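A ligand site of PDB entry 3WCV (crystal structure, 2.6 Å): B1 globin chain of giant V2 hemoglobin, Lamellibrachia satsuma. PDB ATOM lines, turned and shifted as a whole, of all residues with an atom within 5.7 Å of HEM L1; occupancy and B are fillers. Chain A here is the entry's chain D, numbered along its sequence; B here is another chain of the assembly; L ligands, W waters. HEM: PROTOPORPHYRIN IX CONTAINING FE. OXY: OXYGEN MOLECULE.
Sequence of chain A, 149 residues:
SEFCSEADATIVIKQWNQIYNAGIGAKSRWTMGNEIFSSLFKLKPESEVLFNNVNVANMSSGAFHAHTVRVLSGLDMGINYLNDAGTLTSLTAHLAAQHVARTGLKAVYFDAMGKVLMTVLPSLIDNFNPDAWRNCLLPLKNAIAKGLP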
ATOM      1  N   PHE A  37      -7.174 -19.362  -5.416  1.00  0.00           N
ATOM      2  CA  PHE A  37      -8.081 -20.360  -4.860  1.00  0.00           C
ATOM      3  C   PHE A  37      -7.594 -21.795  -5.097  1.00  0.00           C
ATOM      4  O   PHE A  37      -7.651 -22.611  -4.169  1.00  0.00           O
ATOM      5  CB  PHE A  37      -9.491 -20.135  -5.406  1.00  0.00           C
ATOM      6  CG  PHE A  37     -10.205 -18.997  -4.754  1.00  0.00           C
ATOM      7  CD1 PHE A  37     -10.857 -19.185  -3.543  1.00  0.00           C
ATOM      8  CD2 PHE A  37     -10.141 -17.711  -5.284  1.00  0.00           C
ATOM      9  CE1 PHE A  37     -11.444 -18.107  -2.872  1.00  0.00           C
ATOM     10  CE2 PHE A  37     -10.721 -16.637  -4.625  1.00  0.00           C
ATOM     11  CZ  PHE A  37     -11.373 -16.825  -3.414  1.00  0.00           C
ATOM     12  N   LEU A  40      -5.558 -22.420  -2.399  1.00  0.00           N
ATOM     13  CA  LEU A  40      -6.269 -22.505  -1.136  1.00  0.00           C
ATOM     14  C   LEU A  40      -6.895 -23.896  -0.998  1.00  0.00           C
ATOM     15  O   LEU A  40      -6.969 -24.451   0.094  1.00  0.00           O
ATOM     16  CB  LEU A  40      -7.376 -21.453  -1.062  1.00  0.00           C
ATOM     17  CG  LEU A  40      -8.214 -21.577   0.222  1.00  0.00           C
ATOM     18  CD1 LEU A  40      -7.363 -21.190   1.411  1.00  0.00           C
ATOM     19  CD2 LEU A  40      -9.441 -20.689   0.154  1.00  0.00           C
ATOM     20  N   SER A  47     -12.362 -26.850   2.048  1.00  0.00           N
ATOM     21  CA  SER A  47     -13.019 -25.554   1.831  1.00  0.00           C
ATOM     22  C   SER A  47     -13.532 -25.316   0.421  1.00  0.00           C
ATOM     23  O   SER A  47     -14.326 -24.394   0.212  1.00  0.00           O
ATOM     24  CB  SER A  47     -12.066 -24.422   2.210  1.00  0.00           C
ATOM     25  OG  SER A  47     -10.954 -24.376   1.338  1.00  0.00           O
ATOM     26  N   LEU A  50     -17.314 -24.900  -0.197  1.00  0.00           N
ATOM     27  CA  LEU A  50     -17.965 -23.646   0.183  1.00  0.00           C
ATOM     28  C   LEU A  50     -18.316 -22.749  -1.007  1.00  0.00           C
ATOM     29  O   LEU A  50     -19.180 -21.883  -0.900  1.00  0.00           O
ATOM     30  CB  LEU A  50     -17.068 -22.862   1.158  1.00  0.00           C
ATOM     31  CG  LEU A  50     -16.591 -23.576   2.419  1.00  0.00           C
ATOM     32  CD1 LEU A  50     -15.708 -22.638   3.227  1.00  0.00           C
ATOM     33  CD2 LEU A  50     -17.769 -24.022   3.247  1.00  0.00           C
ATOM     34  N   PHE A  51     -17.657 -22.963  -2.132  1.00  0.00           N
ATOM     35  CA  PHE A  51     -17.898 -22.152  -3.324  1.00  0.00           C
ATOM     36  C   PHE A  51     -18.782 -22.813  -4.380  1.00  0.00           C
ATOM     37  O   PHE A  51     -18.867 -22.329  -5.504  1.00  0.00           O
ATOM     38  CB  PHE A  51     -16.562 -21.750  -3.948  1.00  0.00           C
ATOM     39  CG  PHE A  51     -15.657 -21.010  -3.007  1.00  0.00           C
ATOM     40  CD1 PHE A  51     -14.717 -21.682  -2.231  1.00  0.00           C
ATOM     41  CD2 PHE A  51     -15.816 -19.631  -2.829  1.00  0.00           C
ATOM     42  CE1 PHE A  51     -13.940 -21.007  -1.295  1.00  0.00           C
ATOM     43  CE2 PHE A  51     -15.052 -18.949  -1.894  1.00  0.00           C
ATOM     44  CZ  PHE A  51     -14.111 -19.642  -1.129  1.00  0.00           C
ATOM     45  N   ASN A  53     -21.664 -22.617  -4.695  1.00  0.00           N
ATOM     46  CA  ASN A  53     -22.686 -21.650  -5.082  1.00  0.00           C
ATOM     47  C   ASN A  53     -22.277 -20.693  -6.199  1.00  0.00           C
ATOM     48  O   ASN A  53     -23.138 -20.144  -6.889  1.00  0.00           O
ATOM     49  CB  ASN A  53     -23.137 -20.843  -3.878  1.00  0.00           C
ATOM     50  CG  ASN A  53     -24.600 -20.489  -3.939  1.00  0.00           C
ATOM     51  OD1 ASN A  53     -25.467 -21.353  -3.760  1.00  0.00           O
ATOM     52  ND2 ASN A  53     -24.896 -19.224  -4.202  1.00  0.00           N
ATOM     53  N   VAL A  54     -20.971 -20.476  -6.366  1.00  0.00           N
ATOM     54  CA  VAL A  54     -20.450 -19.607  -7.414  1.00  0.00           C
ATOM     55  C   VAL A  54     -19.889 -20.452  -8.557  1.00  0.00           C
ATOM     56  O   VAL A  54     -19.081 -19.984  -9.359  1.00  0.00           O
ATOM     57  CB  VAL A  54     -19.336 -18.670  -6.903  1.00  0.00           C
ATOM     58  CG1 VAL A  54     -19.936 -17.600  -6.015  1.00  0.00           C
ATOM     59  CG2 VAL A  54     -18.301 -19.466  -6.142  1.00  0.00           C
ATOM     60  N   HIS A  67     -16.632 -14.238  -9.135  1.00  0.00           N
ATOM     61  CA  HIS A  67     -16.420 -14.332  -7.705  1.00  0.00           C
ATOM     62  C   HIS A  67     -14.998 -13.875  -7.354  1.00  0.00           C
ATOM     63  O   HIS A  67     -14.810 -13.037  -6.466  1.00  0.00           O
ATOM     64  CB  HIS A  67     -16.644 -15.766  -7.225  1.00  0.00           C
ATOM     65  CG  HIS A  67     -16.230 -15.986  -5.814  1.00  0.00           C
ATOM     66  ND1 HIS A  67     -16.887 -15.399  -4.751  1.00  0.00           N
ATOM     67  CD2 HIS A  67     -15.185 -16.653  -5.274  1.00  0.00           C
ATOM     68  CE1 HIS A  67     -16.265 -15.685  -3.620  1.00  0.00           C
ATOM     69  NE2 HIS A  67     -15.221 -16.456  -3.913  1.00  0.00           N
ATOM     70  N   ARG A  70     -14.605 -10.310  -7.665  1.00  0.00           N
ATOM     71  CA  ARG A  70     -15.211  -9.708  -6.482  1.00  0.00           C
ATOM     72  C   ARG A  70     -14.258  -9.749  -5.287  1.00  0.00           C
ATOM     73  O   ARG A  70     -14.101  -8.773  -4.545  1.00  0.00           O
ATOM     74  CB  ARG A  70     -16.481 -10.500  -6.175  1.00  0.00           C
ATOM     75  CG  ARG A  70     -17.631  -9.714  -5.609  1.00  0.00           C
ATOM     76  CD  ARG A  70     -18.874 -10.597  -5.643  1.00  0.00           C
ATOM     77  NE  ARG A  70     -19.368 -10.774  -7.006  1.00  0.00           N
ATOM     78  CZ  ARG A  70     -19.747 -11.939  -7.507  1.00  0.00           C
ATOM     79  NH1 ARG A  70     -19.688 -13.040  -6.763  1.00  0.00           N
ATOM     80  NH2 ARG A  70     -20.207 -11.999  -8.758  1.00  0.00           N
ATOM     81  N   VAL A  71     -13.630 -10.903  -5.106  1.00  0.00           N
ATOM     82  CA  VAL A  71     -12.704 -11.113  -4.002  1.00  0.00           C
ATOM     83  C   VAL A  71     -11.472 -10.205  -4.078  1.00  0.00           C
ATOM     84  O   VAL A  71     -11.066  -9.594  -3.081  1.00  0.00           O
ATOM     85  CB  VAL A  71     -12.254 -12.599  -3.946  1.00  0.00           C
ATOM     86  CG1 VAL A  71     -11.159 -12.772  -2.923  1.00  0.00           C
ATOM     87  CG2 VAL A  71     -13.451 -13.482  -3.584  1.00  0.00           C
ATOM     88  N   GLY A  74     -12.285  -6.614  -3.398  1.00  0.00           N
ATOM     89  CA  GLY A  74     -12.422  -6.402  -1.965  1.00  0.00           C
ATOM     90  C   GLY A  74     -11.039  -6.211  -1.360  1.00  0.00           C
ATOM     91  O   GLY A  74     -10.786  -5.274  -0.574  1.00  0.00           O
ATOM     92  N   LEU A  75     -10.136  -7.108  -1.733  1.00  0.00           N
ATOM     93  CA  LEU A  75      -8.777  -7.032  -1.260  1.00  0.00           C
ATOM     94  C   LEU A  75      -8.177  -5.674  -1.651  1.00  0.00           C
ATOM     95  O   LEU A  75      -7.494  -5.046  -0.843  1.00  0.00           O
ATOM     96  CB  LEU A  75      -7.958  -8.169  -1.866  1.00  0.00           C
ATOM     97  CG  LEU A  75      -6.466  -8.189  -1.548  1.00  0.00           C
ATOM     98  CD1 LEU A  75      -6.269  -8.016  -0.056  1.00  0.00           C
ATOM     99  CD2 LEU A  75      -5.877  -9.515  -2.013  1.00  0.00           C
ATOM    100  N   LEU A  95     -17.096  -6.766   5.467  1.00  0.00           N
ATOM    101  CA  LEU A  95     -16.568  -7.963   4.807  1.00  0.00           C
ATOM    102  C   LEU A  95     -16.648  -9.112   5.789  1.00  0.00           C
ATOM    103  O   LEU A  95     -16.866 -10.258   5.397  1.00  0.00           O
ATOM    104  CB  LEU A  95     -15.099  -7.771   4.404  1.00  0.00           C
ATOM    105  CG  LEU A  95     -14.791  -7.186   3.034  1.00  0.00           C
ATOM    106  CD1 LEU A  95     -13.333  -6.767   2.922  1.00  0.00           C
ATOM    107  CD2 LEU A  95     -15.117  -8.248   2.011  1.00  0.00           C
ATOM    108  N   GLN A  98     -20.018 -10.534   5.791  1.00  0.00           N
ATOM    109  CA  GLN A  98     -20.276 -11.307   4.584  1.00  0.00           C
ATOM    110  C   GLN A  98     -19.655 -12.696   4.654  1.00  0.00           C
ATOM    111  O   GLN A  98     -19.960 -13.562   3.832  1.00  0.00           O
ATOM    112  CB  GLN A  98     -19.747 -10.577   3.353  1.00  0.00           C
ATOM    113  CG  GLN A  98     -20.464  -9.260   3.033  1.00  0.00           C
ATOM    114  CD  GLN A  98     -19.888  -8.544   1.810  1.00  0.00           C
ATOM    115  OE1 GLN A  98     -18.679  -8.286   1.742  1.00  0.00           O
ATOM    116  NE2 GLN A  98     -20.749  -8.210   0.844  1.00  0.00           N
ATOM    117  N   HIS A  99     -18.773 -12.925   5.625  1.00  0.00           N
ATOM    118  CA  HIS A  99     -18.143 -14.227   5.759  1.00  0.00           C
ATOM    119  C   HIS A  99     -18.700 -15.037   6.912  1.00  0.00           C
ATOM    120  O   HIS A  99     -18.705 -16.270   6.872  1.00  0.00           O
ATOM    121  CB  HIS A  99     -16.625 -14.080   5.870  1.00  0.00           C
ATOM    122  CG  HIS A  99     -15.955 -13.830   4.557  1.00  0.00           C
ATOM    123  ND1 HIS A  99     -15.952 -12.598   3.929  1.00  0.00           N
ATOM    124  CD2 HIS A  99     -15.307 -14.672   3.705  1.00  0.00           C
ATOM    125  CE1 HIS A  99     -15.355 -12.693   2.756  1.00  0.00           C
ATOM    126  NE2 HIS A  99     -14.948 -13.938   2.601  1.00  0.00           N
ATOM    127  N   ARG A 102     -21.784 -17.099   6.370  1.00  0.00           N
ATOM    128  CA  ARG A 102     -21.458 -18.284   5.593  1.00  0.00           C
ATOM    129  C   ARG A 102     -21.027 -19.423   6.505  1.00  0.00           C
ATOM    130  O   ARG A 102     -19.897 -19.450   6.990  1.00  0.00           O
ATOM    131  CB  ARG A 102     -20.336 -17.967   4.591  1.00  0.00           C
ATOM    132  CG  ARG A 102     -20.411 -18.790   3.330  1.00  0.00           C
ATOM    133  CD  ARG A 102     -21.634 -18.407   2.516  1.00  0.00           C
ATOM    134  NE  ARG A 102     -21.684 -19.085   1.226  1.00  0.00           N
ATOM    135  CZ  ARG A 102     -22.398 -18.655   0.182  1.00  0.00           C
ATOM    136  NH1 ARG A 102     -23.114 -17.550   0.279  1.00  0.00           N
ATOM    137  NH2 ARG A 102     -22.383 -19.335  -0.957  1.00  0.00           N
ATOM    138  N   LEU A 105     -17.225 -21.766   7.510  1.00  0.00           N
ATOM    139  CA  LEU A 105     -15.990 -20.990   7.469  1.00  0.00           C
ATOM    140  C   LEU A 105     -15.222 -20.921   8.775  1.00  0.00           C
ATOM    141  O   LEU A 105     -15.698 -20.340   9.760  1.00  0.00           O
ATOM    142  CB  LEU A 105     -16.277 -19.556   7.006  1.00  0.00           C
ATOM    143  CG  LEU A 105     -16.161 -19.323   5.508  1.00  0.00           C
ATOM    144  CD1 LEU A 105     -17.282 -20.060   4.785  1.00  0.00           C
ATOM    145  CD2 LEU A 105     -16.248 -17.841   5.219  1.00  0.00           C
ATOM    146  N   TYR A 109      -9.061 -21.114   7.737  1.00  0.00           N
ATOM    147  CA  TYR A 109      -9.070 -21.000   6.286  1.00  0.00           C
ATOM    148  C   TYR A 109      -8.444 -19.681   5.846  1.00  0.00           C
ATOM    149  O   TYR A 109      -7.863 -19.581   4.765  1.00  0.00           O
ATOM    150  CB  TYR A 109     -10.488 -21.086   5.729  1.00  0.00           C
ATOM    151  CG  TYR A 109     -11.184 -22.404   5.982  1.00  0.00           C
ATOM    152  CD1 TYR A 109     -10.525 -23.608   5.786  1.00  0.00           C
ATOM    153  CD2 TYR A 109     -12.525 -22.425   6.366  1.00  0.00           C
ATOM    154  CE1 TYR A 109     -11.184 -24.832   5.973  1.00  0.00           C
ATOM    155  CE2 TYR A 109     -13.189 -23.628   6.550  1.00  0.00           C
ATOM    156  CZ  TYR A 109     -12.515 -24.833   6.348  1.00  0.00           C
ATOM    157  OH  TYR A 109     -13.174 -26.026   6.515  1.00  0.00           O
ATOM    158  N   PHE A 110      -8.586 -18.665   6.694  1.00  0.00           N
ATOM    159  CA  PHE A 110      -8.022 -17.355   6.407  1.00  0.00           C
ATOM    160  C   PHE A 110      -6.545 -17.357   6.719  1.00  0.00           C
ATOM    161  O   PHE A 110      -5.818 -16.444   6.321  1.00  0.00           O
ATOM    162  CB  PHE A 110      -8.714 -16.264   7.207  1.00  0.00           C
ATOM    163  CG  PHE A 110     -10.006 -15.809   6.601  1.00  0.00           C
ATOM    164  CD1 PHE A 110     -11.126 -16.641   6.635  1.00  0.00           C
ATOM    165  CD2 PHE A 110     -10.110 -14.568   5.993  1.00  0.00           C
ATOM    166  CE1 PHE A 110     -12.328 -16.223   6.061  1.00  0.00           C
ATOM    167  CE2 PHE A 110     -11.312 -14.150   5.419  1.00  0.00           C
ATOM    168  CZ  PHE A 110     -12.420 -14.975   5.449  1.00  0.00           C
ATOM    169  N   MET A 113      -5.305 -18.877   3.460  1.00  0.00           N
ATOM    170  CA  MET A 113      -5.422 -17.835   2.426  1.00  0.00           C
ATOM    171  C   MET A 113      -4.235 -16.883   2.575  1.00  0.00           C
ATOM    172  O   MET A 113      -3.682 -16.416   1.585  1.00  0.00           O
ATOM    173  CB  MET A 113      -6.723 -17.059   2.605  1.00  0.00           C
ATOM    174  CG  MET A 113      -6.893 -15.870   1.673  1.00  0.00           C
ATOM    175  SD  MET A 113      -7.046 -16.264  -0.109  1.00  0.00           S
ATOM    176  CE  MET A 113      -8.753 -16.153  -0.337  1.00  0.00           C
ATOM    177  N   LEU A 117      -1.465 -16.060  -0.322  1.00  0.00           N
ATOM    178  CA  LEU A 117      -1.145 -14.743  -0.801  1.00  0.00           C
ATOM    179  C   LEU A 117       0.359 -14.484  -0.690  1.00  0.00           C
ATOM    180  O   LEU A 117       0.962 -13.940  -1.622  1.00  0.00           O
ATOM    181  CB  LEU A 117      -1.956 -13.665  -0.034  1.00  0.00           C
ATOM    182  CG  LEU A 117      -3.468 -13.692  -0.350  1.00  0.00           C
ATOM    183  CD1 LEU A 117      -4.184 -12.582   0.369  1.00  0.00           C
ATOM    184  CD2 LEU A 117      -3.673 -13.579  -1.851  1.00  0.00           C
ATOM    185  N   LYS A 141      -6.715  -9.533   7.913  1.00  0.00           N
ATOM    186  CA  LYS A 141      -7.203 -10.886   7.985  1.00  0.00           C
ATOM    187  C   LYS A 141      -7.906 -11.160   9.287  1.00  0.00           C
ATOM    188  O   LYS A 141      -8.973 -11.765   9.299  1.00  0.00           O
ATOM    189  CB  LYS A 141      -6.047 -11.853   7.736  1.00  0.00           C
ATOM    190  CG  LYS A 141      -6.462 -13.325   7.693  1.00  0.00           C
ATOM    191  CD  LYS A 141      -6.308 -13.984   9.049  1.00  0.00           C
ATOM    192  CE  LYS A 141      -4.829 -14.096   9.431  1.00  0.00           C
ATOM    193  NZ  LYS A 141      -4.656 -14.714  10.769  1.00  0.00           N
ATOM    194  N   ILE A 144     -11.303  -9.641   9.268  1.00  0.00           N
ATOM    195  CA  ILE A 144     -12.253 -10.314   8.398  1.00  0.00           C
ATOM    196  C   ILE A 144     -12.541 -11.740   8.861  1.00  0.00           C
ATOM    197  O   ILE A 144     -13.528 -12.344   8.435  1.00  0.00           O
ATOM    198  CB  ILE A 144     -11.736 -10.376   6.943  1.00  0.00           C
ATOM    199  CG1 ILE A 144     -11.378  -8.969   6.468  1.00  0.00           C
ATOM    200  CG2 ILE A 144     -12.802 -10.964   6.037  1.00  0.00           C
ATOM    201  CD1 ILE A 144     -10.760  -8.945   5.082  1.00  0.00           C
ATOM    202  N   ARG B  72     -14.877  -2.996 -10.742  1.00  0.00           N
ATOM    203  CA  ARG B  72     -14.783  -4.419 -11.108  1.00  0.00           C
ATOM    204  C   ARG B  72     -15.732  -4.724 -12.271  1.00  0.00           C
ATOM    205  O   ARG B  72     -15.432  -5.569 -13.127  1.00  0.00           O
ATOM    206  CB  ARG B  72     -15.124  -5.295  -9.923  1.00  0.00           C
ATOM    207  CG  ARG B  72     -16.571  -5.240  -9.541  1.00  0.00           C
ATOM    208  CD  ARG B  72     -16.783  -5.997  -8.273  1.00  0.00           C
ATOM    209  NE  ARG B  72     -18.121  -6.567  -8.255  1.00  0.00           N
ATOM    210  CZ  ARG B  72     -18.888  -6.618  -7.182  1.00  0.00           C
ATOM    211  NH1 ARG B  72     -18.423  -6.150  -6.045  1.00  0.00           N
ATOM    212  NH2 ARG B  72     -20.096  -7.116  -7.261  1.00  0.00           N
ATOM    213  N   HIS B  89     -25.263 -10.776  -9.576  1.00  0.00           N
ATOM    214  CA  HIS B  89     -24.889 -10.727  -8.169  1.00  0.00           C
ATOM    215  C   HIS B  89     -25.331  -9.376  -7.572  1.00  0.00           C
ATOM    216  O   HIS B  89     -26.034  -9.306  -6.566  1.00  0.00           O
ATOM    217  CB  HIS B  89     -23.368 -10.896  -8.044  1.00  0.00           C
ATOM    218  CG  HIS B  89     -22.890 -11.056  -6.637  1.00  0.00           C
ATOM    219  ND1 HIS B  89     -22.895 -12.272  -5.990  1.00  0.00           N
ATOM    220  CD2 HIS B  89     -22.438 -10.154  -5.737  1.00  0.00           C
ATOM    221  CE1 HIS B  89     -22.457 -12.122  -4.755  1.00  0.00           C
ATOM    222  NE2 HIS B  89     -22.179 -10.836  -4.574  1.00  0.00           N
ATOM    223  N   GLN B  93     -28.537  -8.189  -4.825  1.00  0.00           N
ATOM    224  CA  GLN B  93     -28.291  -7.362  -3.651  1.00  0.00           C
ATOM    225  C   GLN B  93     -29.127  -6.084  -3.637  1.00  0.00           C
ATOM    226  O   GLN B  93     -29.370  -5.518  -2.574  1.00  0.00           O
ATOM    227  CB  GLN B  93     -26.816  -6.971  -3.547  1.00  0.00           C
ATOM    228  CG  GLN B  93     -25.864  -8.136  -3.329  1.00  0.00           C
ATOM    229  CD  GLN B  93     -24.426  -7.719  -3.401  1.00  0.00           C
ATOM    230  OE1 GLN B  93     -23.971  -7.178  -4.405  1.00  0.00           O
ATOM    231  NE2 GLN B  93     -23.681  -7.985  -2.339  1.00  0.00           N
HETATM  232  CHA HEM L   1     -17.394 -14.063  -0.625  1.00  0.00           C
HETATM  233  CHB HEM L   1     -13.589 -11.274  -0.112  1.00  0.00           C
HETATM  234  CHC HEM L   1     -11.112 -14.895   1.932  1.00  0.00           C
HETATM  235  CHD HEM L   1     -15.035 -17.681   1.467  1.00  0.00           C
HETATM  236  C1A HEM L   1     -16.578 -12.969  -0.667  1.00  0.00           C
HETATM  237  C2A HEM L   1     -16.955 -11.747  -1.230  1.00  0.00           C
HETATM  238  C3A HEM L   1     -15.893 -10.944  -1.085  1.00  0.00           C
HETATM  239  C4A HEM L   1     -14.821 -11.692  -0.428  1.00  0.00           C
HETATM  240  CMA HEM L   1     -15.791  -9.481  -1.527  1.00  0.00           C
HETATM  241  CAA HEM L   1     -18.269 -11.385  -1.871  1.00  0.00           C
HETATM  242  CBA HEM L   1     -19.268 -10.827  -0.921  1.00  0.00           C
HETATM  243  CGA HEM L   1     -20.595 -10.479  -1.574  1.00  0.00           C
HETATM  244  O1A HEM L   1     -21.625 -11.122  -1.262  1.00  0.00           O
HETATM  245  O2A HEM L   1     -20.595  -9.595  -2.386  1.00  0.00           O
HETATM  246  C1B HEM L   1     -12.535 -11.998   0.493  1.00  0.00           C
HETATM  247  C2B HEM L   1     -11.196 -11.446   0.763  1.00  0.00           C
HETATM  248  C3B HEM L   1     -10.467 -12.540   1.355  1.00  0.00           C
HETATM  249  C4B HEM L   1     -11.401 -13.621   1.415  1.00  0.00           C
HETATM  250  CMB HEM L   1     -10.716 -10.082   0.469  1.00  0.00           C
HETATM  251  CAB HEM L   1      -9.066 -12.447   1.779  1.00  0.00           C
HETATM  252  CBB HEM L   1      -8.669 -12.092   2.986  1.00  0.00           C
HETATM  253  C1C HEM L   1     -11.998 -15.971   1.987  1.00  0.00           C
HETATM  254  C2C HEM L   1     -11.612 -17.278   2.564  1.00  0.00           C
HETATM  255  C3C HEM L   1     -12.729 -18.131   2.444  1.00  0.00           C
HETATM  256  C4C HEM L   1     -13.783 -17.253   1.783  1.00  0.00           C
HETATM  257  CMC HEM L   1     -10.234 -17.607   3.149  1.00  0.00           C
HETATM  258  CAC HEM L   1     -12.833 -19.425   2.850  1.00  0.00           C
HETATM  259  CBC HEM L   1     -12.765 -20.605   2.351  1.00  0.00           C
HETATM  260  C1D HEM L   1     -16.032 -16.932   0.847  1.00  0.00           C
HETATM  261  C2D HEM L   1     -17.414 -17.476   0.496  1.00  0.00           C
HETATM  262  C3D HEM L   1     -18.063 -16.429  -0.109  1.00  0.00           C
HETATM  263  C4D HEM L   1     -17.117 -15.294  -0.111  1.00  0.00           C
HETATM  264  CMD HEM L   1     -17.883 -18.890   0.778  1.00  0.00           C
HETATM  265  CAD HEM L   1     -19.477 -16.416  -0.668  1.00  0.00           C
HETATM  266  CBD HEM L   1     -19.499 -16.944  -2.091  1.00  0.00           C
HETATM  267  CGD HEM L   1     -20.824 -16.955  -2.743  1.00  0.00           C
HETATM  268  O1D HEM L   1     -21.348 -15.862  -3.115  1.00  0.00           O
HETATM  269  O2D HEM L   1     -21.389 -18.031  -2.956  1.00  0.00           O
HETATM  270  NA  HEM L   1     -15.265 -12.960  -0.175  1.00  0.00           N
HETATM  271  NB  HEM L   1     -12.669 -13.280   0.860  1.00  0.00           N
HETATM  272  NC  HEM L   1     -13.312 -16.008   1.538  1.00  0.00           N
HETATM  273  ND  HEM L   1     -15.922 -15.641   0.454  1.00  0.00           N
HETATM  274 FE   HEM L   1     -14.296 -14.471   0.698  1.00  0.00          FE
HETATM  275  O1  OXY L   2     -13.697 -14.916  -0.922  1.00  0.00           O
HETATM  276  O2  OXY L   2     -13.724 -16.049  -1.425  1.00  0.00           O
HETATM  277  CHA HEM L   3     -25.179  -1.360  -1.824  1.00  0.00           C
HETATM  278  CHB HEM L   3     -23.125  -1.070  -6.057  1.00  0.00           C
HETATM  279  CHC HEM L   3     -26.498   1.918  -7.575  1.00  0.00           C
HETATM  280  CHD HEM L   3     -28.597   1.597  -3.326  1.00  0.00           C
HETATM  281  C1A HEM L   3     -24.270  -1.581  -2.839  1.00  0.00           C
HETATM  282  C2A HEM L   3     -23.124  -2.394  -2.707  1.00  0.00           C
HETATM  283  C3A HEM L   3     -22.540  -2.327  -3.913  1.00  0.00           C
HETATM  284  C4A HEM L   3     -23.344  -1.440  -4.776  1.00  0.00           C
HETATM  285  CMA HEM L   3     -21.254  -2.990  -4.366  1.00  0.00           C
HETATM  286  CAA HEM L   3     -22.652  -3.164  -1.491  1.00  0.00           C
HETATM  287  CBA HEM L   3     -23.128  -4.587  -1.467  1.00  0.00           C
HETATM  288  CGA HEM L   3     -22.646  -5.388  -0.252  1.00  0.00           C
HETATM  289  O1A HEM L   3     -23.461  -5.729   0.643  1.00  0.00           O
HETATM  290  O2A HEM L   3     -21.479  -5.659  -0.190  1.00  0.00           O
HETATM  291  C1B HEM L   3     -23.849  -0.212  -6.922  1.00  0.00           C
HETATM  292  C2B HEM L   3     -23.465   0.115  -8.296  1.00  0.00           C
HETATM  293  C3B HEM L   3     -24.487   1.003  -8.726  1.00  0.00           C
HETATM  294  C4B HEM L   3     -25.345   1.126  -7.608  1.00  0.00           C
HETATM  295  CMB HEM L   3     -22.277  -0.375  -9.016  1.00  0.00           C
HETATM  296  CAB HEM L   3     -24.530   1.604 -10.033  1.00  0.00           C
HETATM  297  CBB HEM L   3     -24.995   1.020 -11.116  1.00  0.00           C
HETATM  298  C1C HEM L   3     -27.370   2.086  -6.531  1.00  0.00           C
HETATM  299  C2C HEM L   3     -28.558   2.987  -6.638  1.00  0.00           C
HETATM  300  C3C HEM L   3     -29.206   2.917  -5.418  1.00  0.00           C
HETATM  301  C4C HEM L   3     -28.328   1.939  -4.619  1.00  0.00           C
HETATM  302  CMC HEM L   3     -28.940   3.818  -7.887  1.00  0.00           C
HETATM  303  CAC HEM L   3     -30.327   3.575  -5.035  1.00  0.00           C
HETATM  304  CBC HEM L   3     -30.669   4.791  -4.780  1.00  0.00           C
HETATM  305  C1D HEM L   3     -27.851   0.746  -2.509  1.00  0.00           C
HETATM  306  C2D HEM L   3     -28.228   0.434  -1.042  1.00  0.00           C
HETATM  307  C3D HEM L   3     -27.226  -0.416  -0.644  1.00  0.00           C
HETATM  308  C4D HEM L   3     -26.306  -0.588  -1.830  1.00  0.00           C
HETATM  309  CMD HEM L   3     -29.430   0.987  -0.290  1.00  0.00           C
HETATM  310  CAD HEM L   3     -27.052  -1.064   0.713  1.00  0.00           C
HETATM  311  CBD HEM L   3     -26.209  -0.254   1.638  1.00  0.00           C
HETATM  312  CGD HEM L   3     -26.027  -0.935   2.908  1.00  0.00           C
HETATM  313  O1D HEM L   3     -26.733  -0.601   3.908  1.00  0.00           O
HETATM  314  O2D HEM L   3     -25.170  -1.860   2.968  1.00  0.00           O
HETATM  315  NA  HEM L   3     -24.401  -0.997  -4.099  1.00  0.00           N
HETATM  316  NB  HEM L   3     -24.944   0.367  -6.515  1.00  0.00           N
HETATM  317  NC  HEM L   3     -27.285   1.494  -5.313  1.00  0.00           N
HETATM  318  ND  HEM L   3     -26.729   0.126  -2.896  1.00  0.00           N
HETATM  319 FE   HEM L   3     -25.851   0.230  -4.713  1.00  0.00          FE
HETATM  320  O   HOH W   1     -19.255 -14.154  -3.944  1.00  0.00           O
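Water W1 lies within hydrogen-bond range of a ring nitrogen (ND1) of His 67, an oxygen (O1D) of HEM L1 and the guanidinium group of Arg 70.
Leu 40 touches HEM L1 (CD2 to CBC, 3.99 Å).
Ser 47 touches HEM L1 (CB to CBC, 3.9 Å).
Leu 50 touches HEM L1.
CZ of Phe 51 touches CHD of HEM L1, 3.4 Å away.
Asn 53 touches HEM L1 (CB to O2D, 3.4 Å).
Val 54 touches HEM L1.
His 67 touches HEM L1 (CE1 to CHA, 3.6 Å).
Arg 70 touches HEM L1.
Val 71 touches HEM L1.
Leu 75 touches HEM L1.
Leu 95 touches HEM L1.
Gln 98 touches HEM L1 (NE2 to CGA, 3.3 Å).
Leu 105 touches HEM L1.
Tyr 109 touches HEM L1.
Phe 110 touches HEM L1.
CE of Met 113 touches CHC of HEM L1 (3.5 Å).
Hydrophobic or aromatic side chains within 4 Å of HEM L1: Leu 40, Leu 50, Phe 51, Val 54, His 67, Val 71, Leu 95, His 99, Leu 105, Phe 110, Met 113 and His 89 of chain B.
20 residues have an atom within 4 Å of HEM L1: Leu 40, Ser 47, Leu 50, Phe 51, Asn 53, Val 54, His 67, Arg 70, Val 71, Leu 75, Leu 95, Gln 98, His 99, Arg 102, Leu 105, Tyr 109, Phe 110, Met 113, His 89 of chain B and Gln 93 of chain B.
The nearest printed residue that does not touch HEM L1 is Gly 74 (4.3 Å).
A ring nitrogen (ND1) of His 99 lies within hydrogen-bond range of the backbone carbonyl oxygen (O) of Leu 95, 2.9 Å away.
A ring nitrogen (ND1) of His 89 of chain B is in hydrogen-bond range of the guanidinium group (NH1) of Arg 70.
An oxygen (O1) of OXY L2 binds an iron atom (FE) of HEM L1.
An iron atom (FE) of HEM L1 is bound by a ring nitrogen (NE2) of His 99.
The guanidinium group (NH2) of Arg 102 lies within salt-bridge range of an oxygen (O2D) of HEM L1 (2.6 Å).
NE2 of His 89 of chain B lies within hydrogen-bond range of O2A of HEM L1.
NE2 of Gln 93 of chain B is in hydrogen-bond range of O2A of HEM L1.
A ring nitrogen (NE2) of His 67 lies within hydrogen-bond range of an oxygen (O2) of OXY L2, 2.9 Å away.
The side-chain amide nitrogen of Gln 98 sits at hydrogen-bond distance from an oxygen (O2A) of HEM L3, 2.8 Å away.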
